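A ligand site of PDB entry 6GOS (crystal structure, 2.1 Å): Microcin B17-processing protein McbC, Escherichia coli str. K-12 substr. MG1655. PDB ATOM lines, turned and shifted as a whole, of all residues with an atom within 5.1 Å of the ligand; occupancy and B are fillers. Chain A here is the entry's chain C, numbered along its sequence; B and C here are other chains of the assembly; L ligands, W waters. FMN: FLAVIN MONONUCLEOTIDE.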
ATOM      1  N   ARG A  82      -5.530   3.475 -12.908  1.00  0.00           N
ATOM      2  CA  ARG A  82      -6.134   2.172 -13.191  1.00  0.00           C
ATOM      3  C   ARG A  82      -5.969   1.950 -14.677  1.00  0.00           C
ATOM      4  O   ARG A  82      -6.072   2.891 -15.461  1.00  0.00           O
ATOM      5  CB  ARG A  82      -7.611   2.169 -12.801  1.00  0.00           C
ATOM      6  CG  ARG A  82      -8.335   0.860 -13.100  1.00  0.00           C
ATOM      7  CD  ARG A  82      -9.778   0.861 -12.613  1.00  0.00           C
ATOM      8  NE  ARG A  82     -10.516   2.021 -13.106  1.00  0.00           N
ATOM      9  CZ  ARG A  82     -11.217   2.080 -14.242  1.00  0.00           C
ATOM     10  NH1 ARG A  82     -11.314   1.026 -15.046  1.00  0.00           N
ATOM     11  NH2 ARG A  82     -11.842   3.210 -14.564  1.00  0.00           N
ATOM     12  N   LEU A  83      -5.676   0.699 -15.057  1.00  0.00           N
ATOM     13  CA  LEU A  83      -5.494   0.356 -16.476  1.00  0.00           C
ATOM     14  C   LEU A  83      -6.857   0.390 -17.178  1.00  0.00           C
ATOM     15  O   LEU A  83      -7.859  -0.019 -16.562  1.00  0.00           O
ATOM     16  CB  LEU A  83      -4.861  -1.029 -16.641  1.00  0.00           C
ATOM     17  CG  LEU A  83      -3.387  -1.146 -16.259  1.00  0.00           C
ATOM     18  CD1 LEU A  83      -2.957  -2.600 -16.163  1.00  0.00           C
ATOM     19  CD2 LEU A  83      -2.481  -0.395 -17.241  1.00  0.00           C
ATOM     20  N   PRO A  84      -6.888   0.821 -18.463  1.00  0.00           N
ATOM     21  CA  PRO A  84      -8.136   0.725 -19.197  1.00  0.00           C
ATOM     22  C   PRO A  84      -8.642  -0.701 -19.143  1.00  0.00           C
ATOM     23  O   PRO A  84      -7.826  -1.628 -19.070  1.00  0.00           O
ATOM     24  CB  PRO A  84      -7.752   1.132 -20.621  1.00  0.00           C
ATOM     25  CG  PRO A  84      -6.545   1.995 -20.449  1.00  0.00           C
ATOM     26  CD  PRO A  84      -5.811   1.438 -19.267  1.00  0.00           C
ATOM     27  N   SER A  85      -9.966  -0.888 -19.111  1.00  0.00           N
ATOM     28  CA  SER A  85     -10.530  -2.235 -19.045  1.00  0.00           C
ATOM     29  C   SER A  85     -10.242  -2.943 -20.347  1.00  0.00           C
ATOM     30  O   SER A  85     -10.433  -2.367 -21.404  1.00  0.00           O
ATOM     31  CB  SER A  85     -12.028  -2.229 -18.790  1.00  0.00           C
ATOM     32  OG  SER A  85     -12.339  -1.678 -17.526  1.00  0.00           O
ATOM     33  N   ILE A  87     -10.360  -5.385 -23.629  1.00  0.00           N
ATOM     34  CA  ILE A  87     -11.388  -5.708 -24.617  1.00  0.00           C
ATOM     35  C   ILE A  87     -10.675  -6.312 -25.803  1.00  0.00           C
ATOM     36  O   ILE A  87      -9.474  -6.123 -25.941  1.00  0.00           O
ATOM     37  CB  ILE A  87     -12.235  -4.450 -24.968  1.00  0.00           C
ATOM     38  CG1 ILE A  87     -13.597  -4.830 -25.572  1.00  0.00           C
ATOM     39  CG2 ILE A  87     -11.447  -3.475 -25.860  1.00  0.00           C
ATOM     40  CD1 ILE A  87     -14.487  -5.680 -24.675  1.00  0.00           C
ATOM     41  N   ASP A 178     -22.373 -10.039 -27.054  1.00  0.00           N
ATOM     42  CA  ASP A 178     -21.290  -9.135 -27.458  1.00  0.00           C
ATOM     43  C   ASP A 178     -19.928  -9.832 -27.447  1.00  0.00           C
ATOM     44  O   ASP A 178     -18.897  -9.212 -27.169  1.00  0.00           O
ATOM     45  CB  ASP A 178     -21.288  -7.916 -26.518  1.00  0.00           C
ATOM     46  CG  ASP A 178     -20.484  -6.726 -27.066  1.00  0.00           C
ATOM     47  OD1 ASP A 178     -20.382  -6.565 -28.305  1.00  0.00           O
ATOM     48  OD2 ASP A 178     -19.970  -5.948 -26.239  1.00  0.00           O
ATOM     49  N   ARG A 181     -16.817  -8.644 -29.882  1.00  0.00           N
ATOM     50  CA  ARG A 181     -16.108  -7.486 -29.323  1.00  0.00           C
ATOM     51  C   ARG A 181     -15.290  -7.883 -28.112  1.00  0.00           C
ATOM     52  O   ARG A 181     -14.180  -7.391 -27.935  1.00  0.00           O
ATOM     53  CB  ARG A 181     -17.092  -6.373 -28.966  1.00  0.00           C
ATOM     54  CG  ARG A 181     -16.488  -5.186 -28.227  1.00  0.00           C
ATOM     55  CD  ARG A 181     -17.471  -4.026 -28.100  1.00  0.00           C
ATOM     56  NE  ARG A 181     -17.015  -3.106 -27.056  1.00  0.00           N
ATOM     57  CZ  ARG A 181     -17.233  -3.261 -25.756  1.00  0.00           C
ATOM     58  NH1 ARG A 181     -17.935  -4.290 -25.295  1.00  0.00           N
ATOM     59  NH2 ARG A 181     -16.752  -2.367 -24.893  1.00  0.00           N
ATOM     60  N   TYR A 218     -15.041  -7.191  -6.603  1.00  0.00           N
ATOM     61  CA  TYR A 218     -14.459  -7.029  -7.929  1.00  0.00           C
ATOM     62  C   TYR A 218     -13.431  -5.916  -7.993  1.00  0.00           C
ATOM     63  O   TYR A 218     -12.510  -5.989  -8.825  1.00  0.00           O
ATOM     64  CB  TYR A 218     -15.495  -6.938  -9.073  1.00  0.00           C
ATOM     65  CG  TYR A 218     -16.382  -5.718  -9.237  1.00  0.00           C
ATOM     66  CD1 TYR A 218     -15.859  -4.445  -9.479  1.00  0.00           C
ATOM     67  CD2 TYR A 218     -17.777  -5.853  -9.267  1.00  0.00           C
ATOM     68  CE1 TYR A 218     -16.701  -3.353  -9.674  1.00  0.00           C
ATOM     69  CE2 TYR A 218     -18.609  -4.754  -9.470  1.00  0.00           C
ATOM     70  CZ  TYR A 218     -18.065  -3.509  -9.682  1.00  0.00           C
ATOM     71  OH  TYR A 218     -18.878  -2.414  -9.875  1.00  0.00           O
ATOM     72  N   ARG A 233     -12.133  -6.874 -17.332  1.00  0.00           N
ATOM     73  CA  ARG A 233     -13.344  -6.101 -17.588  1.00  0.00           C
ATOM     74  C   ARG A 233     -14.534  -6.684 -16.788  1.00  0.00           C
ATOM     75  O   ARG A 233     -14.908  -7.848 -16.958  1.00  0.00           O
ATOM     76  CB  ARG A 233     -13.667  -6.050 -19.088  1.00  0.00           C
ATOM     77  CG  ARG A 233     -14.917  -5.234 -19.423  1.00  0.00           C
ATOM     78  CD  ARG A 233     -15.130  -4.966 -20.906  1.00  0.00           C
ATOM     79  NE  ARG A 233     -14.175  -4.000 -21.438  1.00  0.00           N
ATOM     80  CZ  ARG A 233     -14.378  -2.705 -21.687  1.00  0.00           C
ATOM     81  NH1 ARG A 233     -15.555  -2.117 -21.481  1.00  0.00           N
ATOM     82  NH2 ARG A 233     -13.376  -1.975 -22.152  1.00  0.00           N
ATOM     83  N   VAL A 234     -15.084  -5.877 -15.898  1.00  0.00           N
ATOM     84  CA  VAL A 234     -16.400  -6.158 -15.289  1.00  0.00           C
ATOM     85  C   VAL A 234     -17.434  -6.110 -16.401  1.00  0.00           C
ATOM     86  O   VAL A 234     -17.346  -5.280 -17.310  1.00  0.00           O
ATOM     87  CB  VAL A 234     -16.735  -5.137 -14.159  1.00  0.00           C
ATOM     88  CG1 VAL A 234     -17.996  -5.570 -13.408  1.00  0.00           C
ATOM     89  CG2 VAL A 234     -15.567  -4.992 -13.196  1.00  0.00           C
ATOM     90  N   TRP A 235     -18.415  -6.985 -16.330  1.00  0.00           N
ATOM     91  CA  TRP A 235     -19.241  -7.312 -17.460  1.00  0.00           C
ATOM     92  C   TRP A 235     -20.650  -7.661 -17.012  1.00  0.00           C
ATOM     93  O   TRP A 235     -20.849  -8.527 -16.185  1.00  0.00           O
ATOM     94  CB  TRP A 235     -18.619  -8.515 -18.134  1.00  0.00           C
ATOM     95  CG  TRP A 235     -19.239  -8.910 -19.397  1.00  0.00           C
ATOM     96  CD1 TRP A 235     -20.184  -9.877 -19.571  1.00  0.00           C
ATOM     97  CD2 TRP A 235     -18.900  -8.432 -20.695  1.00  0.00           C
ATOM     98  NE1 TRP A 235     -20.459 -10.024 -20.910  1.00  0.00           N
ATOM     99  CE2 TRP A 235     -19.696  -9.139 -21.624  1.00  0.00           C
ATOM    100  CE3 TRP A 235     -18.011  -7.464 -21.168  1.00  0.00           C
ATOM    101  CZ2 TRP A 235     -19.643  -8.890 -22.997  1.00  0.00           C
ATOM    102  CZ3 TRP A 235     -17.945  -7.226 -22.560  1.00  0.00           C
ATOM    103  CH2 TRP A 235     -18.763  -7.939 -23.445  1.00  0.00           C
ATOM    104  N   ALA A 236     -21.619  -6.977 -17.589  1.00  0.00           N
ATOM    105  CA  ALA A 236     -23.011  -7.171 -17.292  1.00  0.00           C
ATOM    106  C   ALA A 236     -23.802  -7.740 -18.464  1.00  0.00           C
ATOM    107  O   ALA A 236     -24.993  -8.042 -18.313  1.00  0.00           O
ATOM    108  CB  ALA A 236     -23.599  -5.843 -16.833  1.00  0.00           C
ATOM    109  N   GLY A 237     -23.151  -7.935 -19.598  1.00  0.00           N
ATOM    110  CA  GLY A 237     -23.805  -8.437 -20.809  1.00  0.00           C
ATOM    111  C   GLY A 237     -23.930  -9.948 -20.897  1.00  0.00           C
ATOM    112  O   GLY A 237     -23.336 -10.595 -21.770  1.00  0.00           O
ATOM    113  N   ILE A 258     -22.748 -10.325 -11.279  1.00  0.00           N
ATOM    114  CA  ILE A 258     -21.821  -9.735 -12.208  1.00  0.00           C
ATOM    115  C   ILE A 258     -20.708 -10.732 -12.550  1.00  0.00           C
ATOM    116  O   ILE A 258     -20.307 -11.561 -11.728  1.00  0.00           O
ATOM    117  CB  ILE A 258     -21.240  -8.395 -11.644  1.00  0.00           C
ATOM    118  CG1 ILE A 258     -20.692  -7.492 -12.760  1.00  0.00           C
ATOM    119  CG2 ILE A 258     -20.184  -8.648 -10.576  1.00  0.00           C
ATOM    120  CD1 ILE A 258     -21.749  -6.769 -13.574  1.00  0.00           C
ATOM    121  N   GLY B  63     -25.086  -6.882 -25.695  1.00  0.00           N
ATOM    122  CA  GLY B  63     -24.202  -6.198 -24.709  1.00  0.00           C
ATOM    123  C   GLY B  63     -24.761  -6.126 -23.298  1.00  0.00           C
ATOM    124  O   GLY B  63     -25.783  -6.741 -22.985  1.00  0.00           O
ATOM    125  N   F6N B  64     -24.041  -5.338 -22.403  1.00  0.00           N
ATOM    126  CA1 F6N B  64     -24.603  -4.769 -21.166  1.00  0.00           C
ATOM    127  C2  F6N B  64     -23.738  -3.697 -20.564  1.00  0.00           C
ATOM    128  N2  F6N B  64     -22.828  -3.044 -21.195  1.00  0.00           N
ATOM    129  CA2 F6N B  64     -22.248  -2.167 -20.283  1.00  0.00           C
ATOM    130  C   F6N B  64     -21.107  -1.258 -20.682  1.00  0.00           C
ATOM    131  O   F6N B  64     -20.534  -0.609 -19.805  1.00  0.00           O
ATOM    132  C5  F6N B  64     -22.899  -2.357 -19.080  1.00  0.00           C
ATOM    133  O3  F6N B  64     -23.833  -3.331 -19.259  1.00  0.00           O
ATOM    134  N   GLY B  65     -20.733  -1.259 -21.982  1.00  0.00           N
ATOM    135  CA  GLY B  65     -19.561  -0.501 -22.475  1.00  0.00           C
ATOM    136  C   GLY B  65     -19.960   0.952 -22.582  1.00  0.00           C
ATOM    137  O   GLY B  65     -21.137   1.270 -22.437  1.00  0.00           O
ATOM    138  N   SER B  66     -18.987   1.822 -22.821  1.00  0.00           N
ATOM    139  CA  SER B  66     -19.247   3.208 -23.249  1.00  0.00           C
ATOM    140  C   SER B  66     -19.286   3.283 -24.802  1.00  0.00           C
ATOM    141  O   SER B  66     -19.006   2.290 -25.469  1.00  0.00           O
ATOM    142  CB  SER B  66     -18.164   4.139 -22.697  1.00  0.00           C
ATOM    143  OG  SER B  66     -16.901   3.926 -23.341  1.00  0.00           O
ATOM    144  N   ARG C 117     -10.646   9.499 -16.532  1.00  0.00           N
ATOM    145  CA  ARG C 117     -10.742   8.115 -16.071  1.00  0.00           C
ATOM    146  C   ARG C 117     -10.505   8.020 -14.576  1.00  0.00           C
ATOM    147  O   ARG C 117      -9.592   8.629 -14.059  1.00  0.00           O
ATOM    148  CB  ARG C 117      -9.779   7.216 -16.836  1.00  0.00           C
ATOM    149  CG  ARG C 117     -10.150   7.018 -18.326  1.00  0.00           C
ATOM    150  CD  ARG C 117      -9.410   5.880 -19.042  1.00  0.00           C
ATOM    151  NE  ARG C 117      -9.523   4.600 -18.329  1.00  0.00           N
ATOM    152  CZ  ARG C 117      -8.682   4.160 -17.391  1.00  0.00           C
ATOM    153  NH1 ARG C 117      -7.606   4.871 -17.021  1.00  0.00           N
ATOM    154  NH2 ARG C 117      -8.919   3.003 -16.791  1.00  0.00           N
ATOM    155  N   PRO C 121     -14.175   1.302 -12.093  1.00  0.00           N
ATOM    156  CA  PRO C 121     -14.930   1.272 -13.343  1.00  0.00           C
ATOM    157  C   PRO C 121     -16.412   1.562 -13.125  1.00  0.00           C
ATOM    158  O   PRO C 121     -16.854   1.673 -11.981  1.00  0.00           O
ATOM    159  CB  PRO C 121     -14.743  -0.181 -13.802  1.00  0.00           C
ATOM    160  CG  PRO C 121     -14.701  -0.950 -12.525  1.00  0.00           C
ATOM    161  CD  PRO C 121     -13.955  -0.056 -11.565  1.00  0.00           C
ATOM    162  N   SER C 122     -17.169   1.652 -14.207  1.00  0.00           N
ATOM    163  CA  SER C 122     -18.598   1.993 -14.097  1.00  0.00           C
ATOM    164  C   SER C 122     -19.347   1.571 -15.343  1.00  0.00           C
ATOM    165  O   SER C 122     -18.903   1.854 -16.455  1.00  0.00           O
ATOM    166  CB  SER C 122     -18.801   3.496 -13.914  1.00  0.00           C
ATOM    167  OG  SER C 122     -20.179   3.823 -13.789  1.00  0.00           O
ATOM    168  N   GLY C 123     -20.489   0.932 -15.152  1.00  0.00           N
ATOM    169  CA  GLY C 123     -21.331   0.544 -16.284  1.00  0.00           C
ATOM    170  C   GLY C 123     -21.671   1.736 -17.163  1.00  0.00           C
ATOM    171  O   GLY C 123     -22.125   2.776 -16.668  1.00  0.00           O
ATOM    172  N   GLY C 124     -21.416   1.583 -18.452  1.00  0.00           N
ATOM    173  CA  GLY C 124     -21.636   2.637 -19.427  1.00  0.00           C
ATOM    174  C   GLY C 124     -20.788   3.872 -19.230  1.00  0.00           C
ATOM    175  O   GLY C 124     -21.084   4.903 -19.819  1.00  0.00           O
ATOM    176  N   ALA C 125     -19.741   3.787 -18.399  1.00  0.00           N
ATOM    177  CA  ALA C 125     -19.008   4.964 -17.922  1.00  0.00           C
ATOM    178  C   ALA C 125     -19.971   6.070 -17.417  1.00  0.00           C
ATOM    179  O   ALA C 125     -19.707   7.271 -17.601  1.00  0.00           O
ATOM    180  CB  ALA C 125     -18.104   5.500 -19.037  1.00  0.00           C
ATOM    181  N   TYR C 127     -21.098   6.502 -14.122  1.00  0.00           N
ATOM    182  CA  TYR C 127     -20.746   6.994 -12.768  1.00  0.00           C
ATOM    183  C   TYR C 127     -21.925   7.650 -12.038  1.00  0.00           C
ATOM    184  O   TYR C 127     -21.885   8.846 -11.746  1.00  0.00           O
ATOM    185  CB  TYR C 127     -19.536   7.940 -12.886  1.00  0.00           C
ATOM    186  CG  TYR C 127     -18.318   7.177 -13.317  1.00  0.00           C
ATOM    187  CD1 TYR C 127     -17.594   6.468 -12.370  1.00  0.00           C
ATOM    188  CD2 TYR C 127     -17.943   7.085 -14.661  1.00  0.00           C
ATOM    189  CE1 TYR C 127     -16.501   5.700 -12.724  1.00  0.00           C
ATOM    190  CE2 TYR C 127     -16.832   6.343 -15.034  1.00  0.00           C
ATOM    191  CZ  TYR C 127     -16.111   5.644 -14.046  1.00  0.00           C
ATOM    192  OH  TYR C 127     -15.023   4.859 -14.316  1.00  0.00           O
ATOM    193  N   MET C 209     -26.086  -2.310 -11.021  1.00  0.00           N
ATOM    194  CA  MET C 209     -24.764  -1.762 -11.370  1.00  0.00           C
ATOM    195  C   MET C 209     -24.361  -0.600 -10.461  1.00  0.00           C
ATOM    196  O   MET C 209     -23.179  -0.483 -10.103  1.00  0.00           O
ATOM    197  CB  MET C 209     -24.703  -1.291 -12.853  1.00  0.00           C
ATOM    198  CG  MET C 209     -24.809  -2.387 -13.919  1.00  0.00           C
ATOM    199  SD  MET C 209     -24.787  -1.751 -15.641  1.00  0.00           S
ATOM    200  CE  MET C 209     -26.109  -2.735 -16.312  1.00  0.00           C
ATOM    201  N   MET C 212     -23.430  -1.868  -6.848  1.00  0.00           N
ATOM    202  CA  MET C 212     -22.114  -2.499  -6.973  1.00  0.00           C
ATOM    203  C   MET C 212     -21.004  -1.454  -7.102  1.00  0.00           C
ATOM    204  O   MET C 212     -19.989  -1.530  -6.407  1.00  0.00           O
ATOM    205  CB  MET C 212     -22.079  -3.514  -8.140  1.00  0.00           C
ATOM    206  CG  MET C 212     -22.888  -4.782  -7.851  1.00  0.00           C
ATOM    207  SD  MET C 212     -22.781  -6.108  -9.055  1.00  0.00           S
ATOM    208  CE  MET C 212     -23.389  -5.294 -10.512  1.00  0.00           C
HETATM  209  N1  FMN L   1     -18.030  -3.053 -20.410  1.00  0.00           N
HETATM  210  C2  FMN L   1     -18.506  -3.739 -21.474  1.00  0.00           C
HETATM  211  O2  FMN L   1     -17.909  -3.611 -22.550  1.00  0.00           O
HETATM  212  N3  FMN L   1     -19.596  -4.525 -21.397  1.00  0.00           N
HETATM  213  C4  FMN L   1     -20.255  -4.703 -20.235  1.00  0.00           C
HETATM  214  O4  FMN L   1     -21.259  -5.440 -20.162  1.00  0.00           O
HETATM  215  C4A FMN L   1     -19.802  -3.991 -19.026  1.00  0.00           C
HETATM  216  N5  FMN L   1     -20.439  -4.102 -17.833  1.00  0.00           N
HETATM  217  C5A FMN L   1     -20.002  -3.448 -16.743  1.00  0.00           C
HETATM  218  C6  FMN L   1     -20.686  -3.610 -15.536  1.00  0.00           C
HETATM  219  C7  FMN L   1     -20.263  -2.958 -14.388  1.00  0.00           C
HETATM  220  C7M FMN L   1     -21.003  -3.130 -13.082  1.00  0.00           C
HETATM  221  C8  FMN L   1     -19.072  -2.079 -14.441  1.00  0.00           C
HETATM  222  C8M FMN L   1     -18.631  -1.380 -13.193  1.00  0.00           C
HETATM  223  C9  FMN L   1     -18.380  -1.907 -15.643  1.00  0.00           C
HETATM  224  C9A FMN L   1     -18.781  -2.555 -16.811  1.00  0.00           C
HETATM  225  N10 FMN L   1     -18.101  -2.421 -18.071  1.00  0.00           N
HETATM  226  C10 FMN L   1     -18.602  -3.123 -19.192  1.00  0.00           C
HETATM  227  C1' FMN L   1     -16.897  -1.598 -18.240  1.00  0.00           C
HETATM  228  C2' FMN L   1     -17.243  -0.144 -18.394  1.00  0.00           C
HETATM  229  O2' FMN L   1     -17.804   0.047 -19.693  1.00  0.00           O
HETATM  230  C3' FMN L   1     -15.976   0.674 -18.155  1.00  0.00           C
HETATM  231  O3' FMN L   1     -15.620   0.573 -16.779  1.00  0.00           O
HETATM  232  C4' FMN L   1     -16.144   2.134 -18.549  1.00  0.00           C
HETATM  233  O4' FMN L   1     -16.467   2.212 -19.939  1.00  0.00           O
HETATM  234  C5' FMN L   1     -14.901   2.980 -18.305  1.00  0.00           C
HETATM  235  O5' FMN L   1     -13.803   2.442 -19.034  1.00  0.00           O
HETATM  236  P   FMN L   1     -12.489   1.916 -18.272  1.00  0.00           P
HETATM  237  O1P FMN L   1     -12.955   0.865 -17.281  1.00  0.00           O
HETATM  238  O2P FMN L   1     -11.643   1.341 -19.379  1.00  0.00           O
HETATM  239  O3P FMN L   1     -11.997   3.181 -17.626  1.00  0.00           O
HETATM  240  O   HOH W   1     -15.547   0.564 -22.553  1.00  0.00           O
HETATM  241  O   HOH W   2     -21.005  -5.209 -23.940  1.00  0.00           O
HETATM  242  O   HOH W   3     -14.790   3.356 -21.679  1.00  0.00           O
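The backbone carbonyl oxygen (O) of Ser 85 sits at hydrogen-bond distance from the guanidinium group (NH2) of Arg 233 (3.1 Å). The guanidinium group (NH1) of Arg 117 of chain C is in hydrogen-bond range of the backbone carbonyl oxygen (O) of Arg 82, 3.0 Å away. O of F6N 64 of chain B is in hydrogen-bond range of the backbone NH (N) of Gly 124 of chain C, 2.7 Å away. OD2 of Asp 178 lies within salt-bridge range of NH1 of Arg 181 (2.8 Å). O of Leu 83 is in hydrogen-bond range of NH2 of Arg 117 of chain C (3.2 Å). The indole nitrogen (NE1) of Trp 235 sits at hydrogen-bond distance from the backbone carbonyl oxygen (O) of Gly 237 (3.1 Å). OG of Ser 122 of chain C sits at hydrogen-bond distance from N of Tyr 127 of chain C, at 2.9 Å.
The backbone carbonyl oxygen (O) of Val 234 sits close to a nitrogen (N10) of the ligand, at 3.1 Å. Pro 84 touches the ligand. Tyr 218 touches the ligand. CE3 of Trp 235 touches N3 of the ligand, at 3.3 Å. CD1 of Ile 258 touches C7M of the ligand, 3.7 Å away. Gly 65 of chain B touches the ligand. Ser 66 of chain B touches the ligand (CB to O4', 3.8 Å). CB of Pro 121 of chain C touches O3' of the ligand, at 3.2 Å. N of Gly 123 of chain C touches C8 of the ligand (3.4 Å). CB of Ala 125 of chain C touches O4' of the ligand (3.8 Å). CG of Met 209 of chain C touches C7M of the ligand (3.97 Å). Hydrophobic or aromatic side chains within 4 Å of the ligand: Val 234, Trp 235, Ala 236, Ile 258, Pro 121 of chain C, Ala 125 of chain C and Met 209 of chain C.
Water W3 bridges an oxygen (O4') of the ligand (2.7 Å) and the side-chain hydroxyl (OG) of Ser 66 of chain B (2.7 Å). Water W1 bridges NH1 of Arg 233 (2.9 Å) and O4' of the ligand (3.2 Å).
An oxygen (O2P) of the ligand lies within hydrogen-bond range of the backbone NH of Ser 85 (2.8 Å). The side-chain hydroxyl of Ser 85 lies within hydrogen-bond range of an oxygen (O1P) of the ligand. NH1 of Arg 82 is in salt-bridge range of O1P of the ligand (2.8 Å). O of F6N 64 of chain B is in hydrogen-bond range of O2' of the ligand. The guanidinium group (NH1) of Arg 181 sits at hydrogen-bond distance from an oxygen (O2) of the ligand (2.8 Å). NH1 of Arg 233 is in hydrogen-bond range of N1 of the ligand, 2.9 Å away. An oxygen (O3P) of the ligand is in salt-bridge range of the guanidinium group (NE) of Arg 117 of chain C (2.9 Å). N of Ala 236 is in hydrogen-bond range of O4 of the ligand, at 3.0 Å. The backbone NH (N) of Gly 237 sits at hydrogen-bond distance from an oxygen (O4) of the ligand (3.2 Å). N of Ser 122 of chain C is in hydrogen-bond range of O3' of the ligand.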
